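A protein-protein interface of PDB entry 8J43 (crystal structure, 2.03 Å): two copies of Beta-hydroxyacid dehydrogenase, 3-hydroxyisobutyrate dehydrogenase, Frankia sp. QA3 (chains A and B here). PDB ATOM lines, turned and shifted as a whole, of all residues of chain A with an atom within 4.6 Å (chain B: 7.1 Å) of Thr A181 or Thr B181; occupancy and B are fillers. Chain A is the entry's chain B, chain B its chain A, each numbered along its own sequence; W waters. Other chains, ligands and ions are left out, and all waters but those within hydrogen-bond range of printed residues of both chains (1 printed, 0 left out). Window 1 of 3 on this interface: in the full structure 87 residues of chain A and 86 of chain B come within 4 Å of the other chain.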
ATOM      1  N   LEU A 177      -3.144  30.657 -15.252  1.00  0.00           N
ATOM      2  CA  LEU A 177      -2.535  29.372 -15.584  1.00  0.00           C
ATOM      3  C   LEU A 177      -2.873  28.287 -14.544  1.00  0.00           C
ATOM      4  O   LEU A 177      -3.258  27.172 -14.904  1.00  0.00           O
ATOM      5  CB  LEU A 177      -1.008  29.528 -15.753  1.00  0.00           C
ATOM      6  CG  LEU A 177      -0.219  28.246 -16.065  1.00  0.00           C
ATOM      7  CD1 LEU A 177      -0.849  27.505 -17.229  1.00  0.00           C
ATOM      8  CD2 LEU A 177       1.233  28.559 -16.367  1.00  0.00           C
ATOM      9  N   MET A 178      -2.746  28.606 -13.259  1.00  0.00           N
ATOM     10  CA  MET A 178      -2.976  27.615 -12.197  1.00  0.00           C
ATOM     11  C   MET A 178      -4.432  27.208 -12.148  1.00  0.00           C
ATOM     12  O   MET A 178      -4.731  26.028 -12.109  1.00  0.00           O
ATOM     13  CB  MET A 178      -2.540  28.116 -10.825  1.00  0.00           C
ATOM     14  CG  MET A 178      -3.013  27.232  -9.663  1.00  0.00           C
ATOM     15  SD  MET A 178      -3.007  28.052  -8.051  1.00  0.00           S
ATOM     16  CE  MET A 178      -4.458  29.084  -8.243  1.00  0.00           C
ATOM     17  N   TRP A 179      -5.335  28.174 -12.118  1.00  0.00           N
ATOM     18  CA  TRP A 179      -6.773  27.856 -12.121  1.00  0.00           C
ATOM     19  C   TRP A 179      -7.182  27.052 -13.362  1.00  0.00           C
ATOM     20  O   TRP A 179      -7.985  26.126 -13.279  1.00  0.00           O
ATOM     21  CB  TRP A 179      -7.631  29.113 -12.008  1.00  0.00           C
ATOM     22  CG  TRP A 179      -7.503  29.783 -10.687  1.00  0.00           C
ATOM     23  CD1 TRP A 179      -7.640  29.202  -9.460  1.00  0.00           C
ATOM     24  CD2 TRP A 179      -7.235  31.170 -10.446  1.00  0.00           C
ATOM     25  NE1 TRP A 179      -7.447  30.141  -8.475  1.00  0.00           N
ATOM     26  CE2 TRP A 179      -7.193  31.352  -9.053  1.00  0.00           C
ATOM     27  CE3 TRP A 179      -7.024  32.275 -11.273  1.00  0.00           C
ATOM     28  CZ2 TRP A 179      -6.932  32.600  -8.460  1.00  0.00           C
ATOM     29  CZ3 TRP A 179      -6.767  33.517 -10.677  1.00  0.00           C
ATOM     30  CH2 TRP A 179      -6.721  33.656  -9.291  1.00  0.00           C
ATOM     31  N   SER A 180      -6.618  27.389 -14.513  1.00  0.00           N
ATOM     32  CA  SER A 180      -6.922  26.627 -15.728  1.00  0.00           C
ATOM     33  C   SER A 180      -6.472  25.164 -15.601  1.00  0.00           C
ATOM     34  O   SER A 180      -7.234  24.223 -15.901  1.00  0.00           O
ATOM     35  CB  SER A 180      -6.274  27.279 -16.944  1.00  0.00           C
ATOM     36  OG  SER A 180      -6.688  28.654 -17.063  1.00  0.00           O
ATOM     37  N   THR A 181      -5.240  24.978 -15.139  1.00  0.00           N
ATOM     38  CA  THR A 181      -4.678  23.628 -14.948  1.00  0.00           C
ATOM     39  C   THR A 181      -5.484  22.811 -13.923  1.00  0.00           C
ATOM     40  O   THR A 181      -5.858  21.661 -14.186  1.00  0.00           O
ATOM     41  CB  THR A 181      -3.185  23.720 -14.546  1.00  0.00           C
ATOM     42  OG1 THR A 181      -2.484  24.476 -15.545  1.00  0.00           O
ATOM     43  CG2 THR A 181      -2.558  22.344 -14.418  1.00  0.00           C
ATOM     44  N   LEU A 182      -5.764  23.412 -12.767  1.00  0.00           N
ATOM     45  CA  LEU A 182      -6.507  22.732 -11.695  1.00  0.00           C
ATOM     46  C   LEU A 182      -7.861  22.269 -12.162  1.00  0.00           C
ATOM     47  O   LEU A 182      -8.288  21.163 -11.822  1.00  0.00           O
ATOM     48  CB  LEU A 182      -6.709  23.642 -10.476  1.00  0.00           C
ATOM     49  CG  LEU A 182      -5.453  23.939  -9.663  1.00  0.00           C
ATOM     50  CD1 LEU A 182      -5.684  25.141  -8.761  1.00  0.00           C
ATOM     51  CD2 LEU A 182      -5.066  22.747  -8.830  1.00  0.00           C
ATOM     52  N   THR A 183      -8.554  23.130 -12.913  1.00  0.00           N
ATOM     53  CA  THR A 183      -9.914  22.837 -13.349  1.00  0.00           C
ATOM     54  C   THR A 183      -9.921  21.753 -14.440  1.00  0.00           C
ATOM     55  O   THR A 183     -10.707  20.800 -14.374  1.00  0.00           O
ATOM     56  CB  THR A 183     -10.662  24.128 -13.770  1.00  0.00           C
ATOM     57  OG1 THR A 183     -10.441  25.162 -12.798  1.00  0.00           O
ATOM     58  CG2 THR A 183     -12.172  23.892 -13.812  1.00  0.00           C
ATOM     59  N   GLY A 184      -9.014  21.852 -15.415  1.00  0.00           N
ATOM     60  CA  GLY A 184      -8.848  20.781 -16.394  1.00  0.00           C
ATOM     61  C   GLY A 184      -8.463  19.446 -15.756  1.00  0.00           C
ATOM     62  O   GLY A 184      -8.944  18.371 -16.171  1.00  0.00           O
ATOM     63  N   TRP A 185      -7.600  19.502 -14.739  1.00  0.00           N
ATOM     64  CA  TRP A 185      -7.239  18.306 -13.989  1.00  0.00           C
ATOM     65  C   TRP A 185      -8.453  17.727 -13.299  1.00  0.00           C
ATOM     66  O   TRP A 185      -8.678  16.529 -13.351  1.00  0.00           O
ATOM     67  CB  TRP A 185      -6.160  18.604 -12.950  1.00  0.00           C
ATOM     68  CG  TRP A 185      -5.962  17.492 -11.964  1.00  0.00           C
ATOM     69  CD1 TRP A 185      -5.487  16.241 -12.226  1.00  0.00           C
ATOM     70  CD2 TRP A 185      -6.260  17.520 -10.574  1.00  0.00           C
ATOM     71  NE1 TRP A 185      -5.416  15.503 -11.078  1.00  0.00           N
ATOM     72  CE2 TRP A 185      -5.894  16.260 -10.046  1.00  0.00           C
ATOM     73  CE3 TRP A 185      -6.766  18.497  -9.709  1.00  0.00           C
ATOM     74  CZ2 TRP A 185      -6.058  15.943  -8.702  1.00  0.00           C
ATOM     75  CZ3 TRP A 185      -6.917  18.188  -8.377  1.00  0.00           C
ATOM     76  CH2 TRP A 185      -6.573  16.916  -7.884  1.00  0.00           C
ATOM     77  N   LEU A 210       2.448  16.907 -17.186  1.00  0.00           N
ATOM     78  CA  LEU A 210       2.645  18.351 -17.119  1.00  0.00           C
ATOM     79  C   LEU A 210       4.071  18.773 -17.467  1.00  0.00           C
ATOM     80  O   LEU A 210       4.298  19.921 -17.879  1.00  0.00           O
ATOM     81  CB  LEU A 210       2.241  18.897 -15.751  1.00  0.00           C
ATOM     82  CG  LEU A 210       0.759  19.255 -15.631  1.00  0.00           C
ATOM     83  CD1 LEU A 210       0.451  19.577 -14.164  1.00  0.00           C
ATOM     84  CD2 LEU A 210       0.380  20.413 -16.569  1.00  0.00           C
ATOM     85  N   VAL A 213       3.872  19.002 -21.160  1.00  0.00           N
ATOM     86  CA  VAL A 213       3.069  20.171 -21.495  1.00  0.00           C
ATOM     87  C   VAL A 213       3.894  21.447 -21.286  1.00  0.00           C
ATOM     88  O   VAL A 213       3.819  22.365 -22.101  1.00  0.00           O
ATOM     89  CB  VAL A 213       1.792  20.255 -20.633  1.00  0.00           C
ATOM     90  CG1 VAL A 213       1.060  21.580 -20.866  1.00  0.00           C
ATOM     91  CG2 VAL A 213       0.870  19.090 -20.957  1.00  0.00           C
ATOM     92  N   LEU B 175      -5.521  15.102 -22.155  1.00  0.00           N
ATOM     93  CA  LEU B 175      -5.610  16.145 -23.184  1.00  0.00           C
ATOM     94  C   LEU B 175      -6.379  17.389 -22.688  1.00  0.00           C
ATOM     95  O   LEU B 175      -5.961  18.532 -22.922  1.00  0.00           O
ATOM     96  CB  LEU B 175      -6.215  15.597 -24.472  1.00  0.00           C
ATOM     97  CG  LEU B 175      -5.314  14.593 -25.181  1.00  0.00           C
ATOM     98  CD1 LEU B 175      -6.009  13.997 -26.389  1.00  0.00           C
ATOM     99  CD2 LEU B 175      -4.002  15.247 -25.589  1.00  0.00           C
ATOM    100  N   GLY B 176      -7.475  17.149 -21.974  1.00  0.00           N
ATOM    101  CA  GLY B 176      -8.262  18.239 -21.380  1.00  0.00           C
ATOM    102  C   GLY B 176      -7.436  19.116 -20.450  1.00  0.00           C
ATOM    103  O   GLY B 176      -7.513  20.361 -20.499  1.00  0.00           O
ATOM    104  N   LEU B 177      -6.654  18.450 -19.592  1.00  0.00           N
ATOM    105  CA  LEU B 177      -5.633  19.110 -18.796  1.00  0.00           C
ATOM    106  C   LEU B 177      -4.687  19.961 -19.675  1.00  0.00           C
ATOM    107  O   LEU B 177      -4.407  21.120 -19.351  1.00  0.00           O
ATOM    108  CB  LEU B 177      -4.852  18.066 -17.963  1.00  0.00           C
ATOM    109  CG  LEU B 177      -3.676  18.591 -17.127  1.00  0.00           C
ATOM    110  CD1 LEU B 177      -4.103  19.777 -16.289  1.00  0.00           C
ATOM    111  CD2 LEU B 177      -3.089  17.516 -16.247  1.00  0.00           C
ATOM    112  N   MET B 178      -4.207  19.399 -20.782  1.00  0.00           N
ATOM    113  CA  MET B 178      -3.247  20.103 -21.645  1.00  0.00           C
ATOM    114  C   MET B 178      -3.881  21.309 -22.297  1.00  0.00           C
ATOM    115  O   MET B 178      -3.297  22.389 -22.269  1.00  0.00           O
ATOM    116  CB  MET B 178      -2.662  19.193 -22.731  1.00  0.00           C
ATOM    117  CG  MET B 178      -1.851  19.936 -23.790  1.00  0.00           C
ATOM    118  SD  MET B 178      -1.662  19.015 -25.337  1.00  0.00           S
ATOM    119  CE  MET B 178      -3.300  19.197 -26.035  1.00  0.00           C
ATOM    120  N   TRP B 179      -5.045  21.133 -22.919  1.00  0.00           N
ATOM    121  CA  TRP B 179      -5.748  22.261 -23.531  1.00  0.00           C
ATOM    122  C   TRP B 179      -6.053  23.373 -22.530  1.00  0.00           C
ATOM    123  O   TRP B 179      -5.926  24.567 -22.841  1.00  0.00           O
ATOM    124  CB  TRP B 179      -7.035  21.827 -24.231  1.00  0.00           C
ATOM    125  CG  TRP B 179      -6.780  21.000 -25.447  1.00  0.00           C
ATOM    126  CD1 TRP B 179      -5.939  21.296 -26.470  1.00  0.00           C
ATOM    127  CD2 TRP B 179      -7.366  19.722 -25.758  1.00  0.00           C
ATOM    128  NE1 TRP B 179      -5.967  20.288 -27.400  1.00  0.00           N
ATOM    129  CE2 TRP B 179      -6.831  19.310 -26.987  1.00  0.00           C
ATOM    130  CE3 TRP B 179      -8.292  18.902 -25.120  1.00  0.00           C
ATOM    131  CZ2 TRP B 179      -7.189  18.096 -27.598  1.00  0.00           C
ATOM    132  CZ3 TRP B 179      -8.656  17.706 -25.730  1.00  0.00           C
ATOM    133  CH2 TRP B 179      -8.109  17.322 -26.956  1.00  0.00           C
ATOM    134  N   SER B 180      -6.442  22.990 -21.322  1.00  0.00           N
ATOM    135  CA  SER B 180      -6.738  23.987 -20.303  1.00  0.00           C
ATOM    136  C   SER B 180      -5.481  24.780 -19.932  1.00  0.00           C
ATOM    137  O   SER B 180      -5.504  26.017 -19.849  1.00  0.00           O
ATOM    138  CB  SER B 180      -7.327  23.312 -19.053  1.00  0.00           C
ATOM    139  OG  SER B 180      -8.479  22.554 -19.375  1.00  0.00           O
ATOM    140  N   THR B 181      -4.385  24.064 -19.706  1.00  0.00           N
ATOM    141  CA  THR B 181      -3.096  24.701 -19.380  1.00  0.00           C
ATOM    142  C   THR B 181      -2.608  25.629 -20.499  1.00  0.00           C
ATOM    143  O   THR B 181      -2.234  26.777 -20.238  1.00  0.00           O
ATOM    144  CB  THR B 181      -2.037  23.624 -19.037  1.00  0.00           C
ATOM    145  OG1 THR B 181      -2.544  22.823 -17.968  1.00  0.00           O
ATOM    146  CG2 THR B 181      -0.714  24.233 -18.629  1.00  0.00           C
ATOM    147  N   LEU B 182      -2.620  25.144 -21.739  1.00  0.00           N
ATOM    148  CA  LEU B 182      -2.152  25.937 -22.886  1.00  0.00           C
ATOM    149  C   LEU B 182      -2.930  27.226 -23.045  1.00  0.00           C
ATOM    150  O   LEU B 182      -2.344  28.263 -23.331  1.00  0.00           O
ATOM    151  CB  LEU B 182      -2.267  25.142 -24.183  1.00  0.00           C
ATOM    152  CG  LEU B 182      -1.201  24.094 -24.404  1.00  0.00           C
ATOM    153  CD1 LEU B 182      -1.629  23.044 -25.423  1.00  0.00           C
ATOM    154  CD2 LEU B 182       0.032  24.810 -24.916  1.00  0.00           C
ATOM    155  N   THR B 183      -4.250  27.144 -22.871  1.00  0.00           N
ATOM    156  CA  THR B 183      -5.124  28.295 -23.061  1.00  0.00           C
ATOM    157  C   THR B 183      -4.940  29.313 -21.912  1.00  0.00           C
ATOM    158  O   THR B 183      -4.796  30.525 -22.152  1.00  0.00           O
ATOM    159  CB  THR B 183      -6.597  27.853 -23.262  1.00  0.00           C
ATOM    160  OG1 THR B 183      -6.662  26.762 -24.196  1.00  0.00           O
ATOM    161  CG2 THR B 183      -7.446  28.991 -23.836  1.00  0.00           C
ATOM    162  N   GLY B 184      -4.883  28.831 -20.673  1.00  0.00           N
ATOM    163  CA  GLY B 184      -4.545  29.707 -19.527  1.00  0.00           C
ATOM    164  C   GLY B 184      -3.177  30.361 -19.664  1.00  0.00           C
ATOM    165  O   GLY B 184      -3.000  31.540 -19.328  1.00  0.00           O
ATOM    166  N   TRP B 185      -2.201  29.589 -20.164  1.00  0.00           N
ATOM    167  CA  TRP B 185      -0.864  30.114 -20.439  1.00  0.00           C
ATOM    168  C   TRP B 185      -0.934  31.202 -21.468  1.00  0.00           C
ATOM    169  O   TRP B 185      -0.323  32.260 -21.283  1.00  0.00           O
ATOM    170  CB  TRP B 185       0.094  29.020 -20.921  1.00  0.00           C
ATOM    171  CG  TRP B 185       1.375  29.563 -21.497  1.00  0.00           C
ATOM    172  CD1 TRP B 185       2.347  30.257 -20.832  1.00  0.00           C
ATOM    173  CD2 TRP B 185       1.801  29.491 -22.852  1.00  0.00           C
ATOM    174  NE1 TRP B 185       3.359  30.593 -21.678  1.00  0.00           N
ATOM    175  CE2 TRP B 185       3.052  30.143 -22.930  1.00  0.00           C
ATOM    176  CE3 TRP B 185       1.259  28.930 -24.008  1.00  0.00           C
ATOM    177  CZ2 TRP B 185       3.767  30.249 -24.120  1.00  0.00           C
ATOM    178  CZ3 TRP B 185       1.973  29.025 -25.186  1.00  0.00           C
ATOM    179  CH2 TRP B 185       3.213  29.683 -25.238  1.00  0.00           C
ATOM    180  N   LEU B 186      -1.639  30.939 -22.566  1.00  0.00           N
ATOM    181  CA  LEU B 186      -1.762  31.921 -23.657  1.00  0.00           C
ATOM    182  C   LEU B 186      -2.479  33.187 -23.195  1.00  0.00           C
ATOM    183  O   LEU B 186      -2.110  34.309 -23.584  1.00  0.00           O
ATOM    184  CB  LEU B 186      -2.497  31.329 -24.864  1.00  0.00           C
ATOM    185  CG  LEU B 186      -1.720  30.290 -25.671  1.00  0.00           C
ATOM    186  CD1 LEU B 186      -2.657  29.588 -26.628  1.00  0.00           C
ATOM    187  CD2 LEU B 186      -0.538  30.914 -26.408  1.00  0.00           C
ATOM    188  N   HIS B 187      -3.518  33.018 -22.391  1.00  0.00           N
ATOM    189  CA  HIS B 187      -4.241  34.184 -21.836  1.00  0.00           C
ATOM    190  C   HIS B 187      -3.308  35.077 -20.999  1.00  0.00           C
ATOM    191  O   HIS B 187      -3.233  36.294 -21.218  1.00  0.00           O
ATOM    192  CB  HIS B 187      -5.422  33.699 -21.004  1.00  0.00           C
ATOM    193  CG  HIS B 187      -6.255  34.791 -20.434  1.00  0.00           C
ATOM    194  ND1 HIS B 187      -5.930  35.440 -19.262  1.00  0.00           N
ATOM    195  CD2 HIS B 187      -7.427  35.322 -20.852  1.00  0.00           C
ATOM    196  CE1 HIS B 187      -6.864  36.334 -18.985  1.00  0.00           C
ATOM    197  NE2 HIS B 187      -7.783  36.285 -19.936  1.00  0.00           N
ATOM    198  N   LEU B 210       4.591  25.729 -12.947  1.00  0.00           N
ATOM    199  CA  LEU B 210       3.848  24.494 -13.180  1.00  0.00           C
ATOM    200  C   LEU B 210       4.329  23.341 -12.298  1.00  0.00           C
ATOM    201  O   LEU B 210       3.568  22.386 -12.046  1.00  0.00           O
ATOM    202  CB  LEU B 210       3.890  24.084 -14.653  1.00  0.00           C
ATOM    203  CG  LEU B 210       2.800  24.714 -15.511  1.00  0.00           C
ATOM    204  CD1 LEU B 210       3.066  24.392 -16.980  1.00  0.00           C
ATOM    205  CD2 LEU B 210       1.398  24.241 -15.083  1.00  0.00           C
ATOM    206  N   VAL B 213       2.383  23.877  -9.201  1.00  0.00           N
ATOM    207  CA  VAL B 213       1.002  23.550  -9.482  1.00  0.00           C
ATOM    208  C   VAL B 213       0.826  22.028  -9.510  1.00  0.00           C
ATOM    209  O   VAL B 213      -0.168  21.515  -8.985  1.00  0.00           O
ATOM    210  CB  VAL B 213       0.519  24.147 -10.815  1.00  0.00           C
ATOM    211  CG1 VAL B 213      -0.881  23.634 -11.157  1.00  0.00           C
ATOM    212  CG2 VAL B 213       0.520  25.678 -10.768  1.00  0.00           C
ATOM    213  N   ALA B 214       1.775  21.313 -10.124  1.00  0.00           N
ATOM    214  CA  ALA B 214       1.694  19.854 -10.171  1.00  0.00           C
ATOM    215  C   ALA B 214       1.671  19.289  -8.745  1.00  0.00           C
ATOM    216  O   ALA B 214       0.999  18.311  -8.479  1.00  0.00           O
ATOM    217  CB  ALA B 214       2.854  19.265 -10.949  1.00  0.00           C
ATOM    218  N   LEU B 217      -1.771  19.361  -7.384  1.00  0.00           N
ATOM    219  CA  LEU B 217      -2.539  18.209  -7.848  1.00  0.00           C
ATOM    220  C   LEU B 217      -2.303  17.003  -6.919  1.00  0.00           C
ATOM    221  O   LEU B 217      -3.249  16.324  -6.515  1.00  0.00           O
ATOM    222  CB  LEU B 217      -2.170  17.820  -9.278  1.00  0.00           C
ATOM    223  CG  LEU B 217      -2.198  18.871 -10.389  1.00  0.00           C
ATOM    224  CD1 LEU B 217      -2.203  18.144 -11.714  1.00  0.00           C
ATOM    225  CD2 LEU B 217      -3.379  19.820 -10.323  1.00  0.00           C
ATOM    226  N   LEU B 259     -12.308  32.723 -20.644  1.00  0.00           N
ATOM    227  CA  LEU B 259     -11.763  31.628 -19.845  1.00  0.00           C
ATOM    228  C   LEU B 259     -11.806  31.929 -18.337  1.00  0.00           C
ATOM    229  O   LEU B 259     -12.451  31.221 -17.598  1.00  0.00           O
ATOM    230  CB  LEU B 259     -10.354  31.212 -20.318  1.00  0.00           C
ATOM    231  CG  LEU B 259      -9.672  30.136 -19.454  1.00  0.00           C
ATOM    232  CD1 LEU B 259     -10.485  28.853 -19.386  1.00  0.00           C
ATOM    233  CD2 LEU B 259      -8.277  29.825 -19.959  1.00  0.00           C
ATOM    234  N   LEU B 263     -13.878  30.146 -15.193  1.00  0.00           N
ATOM    235  CA  LEU B 263     -13.221  29.654 -13.968  1.00  0.00           C
ATOM    236  C   LEU B 263     -13.777  30.342 -12.700  1.00  0.00           C
ATOM    237  O   LEU B 263     -13.963  29.709 -11.665  1.00  0.00           O
ATOM    238  CB  LEU B 263     -11.698  29.820 -14.054  1.00  0.00           C
ATOM    239  CG  LEU B 263     -11.022  29.070 -15.231  1.00  0.00           C
ATOM    240  CD1 LEU B 263      -9.543  29.399 -15.311  1.00  0.00           C
ATOM    241  CD2 LEU B 263     -11.234  27.572 -15.125  1.00  0.00           C
ATOM    242  N   TYR B 280      -9.552  24.328  -3.302  1.00  0.00           N
ATOM    243  CA  TYR B 280      -9.998  24.393  -4.696  1.00  0.00           C
ATOM    244  C   TYR B 280     -10.471  23.022  -5.215  1.00  0.00           C
ATOM    245  O   TYR B 280     -11.319  22.950  -6.104  1.00  0.00           O
ATOM    246  CB  TYR B 280      -8.898  24.973  -5.616  1.00  0.00           C
ATOM    247  CG  TYR B 280      -9.432  25.433  -6.950  1.00  0.00           C
ATOM    248  CD1 TYR B 280      -9.546  24.552  -8.017  1.00  0.00           C
ATOM    249  CD2 TYR B 280      -9.864  26.745  -7.130  1.00  0.00           C
ATOM    250  CE1 TYR B 280     -10.056  24.962  -9.239  1.00  0.00           C
ATOM    251  CE2 TYR B 280     -10.368  27.177  -8.349  1.00  0.00           C
ATOM    252  CZ  TYR B 280     -10.473  26.289  -9.399  1.00  0.00           C
ATOM    253  OH  TYR B 280     -10.986  26.728 -10.604  1.00  0.00           O
HETATM  254  O   HOH W   1       4.842  20.822 -14.591  1.00  0.00           O
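OG1 of Thr A181 lies within hydrogen-bond range of OG1 of Thr B181 (2.9 Å). The side-chain hydroxyl of Tyr B280 sits at hydrogen-bond distance from the side-chain hydroxyl of Thr A183, at 2.8 Å.
The backbone carbonyl oxygen of Gly B176 sits at hydrogen-bond distance from the side-chain hydroxyl of Ser B180 (2.6 Å). The backbone carbonyl oxygen (O) of Leu A177 sits at hydrogen-bond distance from the side-chain hydroxyl (OG1) of Thr A181 (2.9 Å). The side-chain hydroxyl (OG1) of Thr A183 lies within hydrogen-bond range of the backbone carbonyl oxygen (O) of Trp A179 (2.7 Å). The backbone carbonyl oxygen (O) of Leu B177 sits at hydrogen-bond distance from the side-chain hydroxyl (OG1) of Thr B181 (2.9 Å).
Among the printed residues, merely in contact across the chains: Ser A180 with Ser B180 (3.3 Å), Thr A181 with Leu B177 (3.3 Å), Leu A177 with Thr B181 (3.4 Å), Ser A180 with Gly B184 (3.4 Å), Ser A180 with Leu B263 (3.4 Å), Thr A183 with Leu B263 (3.4 Å), Gly A184 with Ser B180 (3.5 Å), Ser A180 with Leu B259 (3.5 Å), Trp A179 with Tyr B280 (3.6 Å), Trp A185 with Leu B217 (3.6 Å), Leu A182 with Leu B217 (3.7 Å), Leu A182 with Tyr B280 (3.8 Å), Trp A179 with Leu B263 (3.8 Å), Trp A185 with Leu B177 (3.8 Å), Leu A177 with Trp B185 (3.8 Å), Leu A210 with Leu B217 (3.9 Å), Thr A181 with Val B213 (3.9 Å), Val A213 with Thr B181 (3.9 Å), Met A178 with Val B213 (3.9 Å), Thr A181 with Leu B210 (3.9 Å) and Val A213 with Met B178 (3.95 Å).
Printed residues of chain B within 4 Å of Trp A179: Leu B263 (3.8 Å) and Tyr B280 (3.6 Å). Thr A181 touches four residues of chain B. Of the printed residues of chain B, Val A213 touches Met B178 and Thr B181. Thr B181 touches three residues of chain A. Of the printed residues of chain A, Val B213 touches Met A178 (3.9 Å) and Thr A181 (3.9 Å). Printed residues of chain A within 4 Å of Leu B259: Ser A180. The nearest residue of chain B that does not touch Thr A181 is Ser B180 (4.7 Å). The nearest residue of chain A that does not touch Thr B181 is Leu A210 (4.04 Å).
Of the 11 printed residues of chain A, 11 touch a printed residue of chain B. Hydrophobic or aromatic side chains of chain A within 4 Å of the printed part of chain B: Leu A177, Met A178, Trp A179, Leu A182, Trp A185, Leu A210 and Val A213. Of the 20 printed residues of chain B, 12 touch a printed residue of chain A. Hydrophobic or aromatic side chains of chain B within 4 Å of the printed part of chain A: Leu B177, Met B178, Leu B210, Val B213, Leu B217, Leu B259, Leu B263 and Tyr B280. Among the printed residues, 23 pairs touch across the chains.
Leu A177 touches Trp B185, and with the chains exchanged Trp A185 touches Leu B177. Met A178 touches Val B213, and with the chains exchanged Val A213 touches Met B178. Ser A180 touches its own counterpart, Ser B180. Thr A181 touches Leu B210, but with the chains exchanged Leu A210 does not touch Thr B181 (4.04 Å). Positions printed for both chains: 177, 178, 179, 180, 181, 182, 183, 184, 185, 210 and 213.
Water W1 bridges the backbone carbonyl oxygen (O) of Leu B210 (3.2 Å) and the backbone carbonyl oxygen (O) of Leu A210 (3.5 Å).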
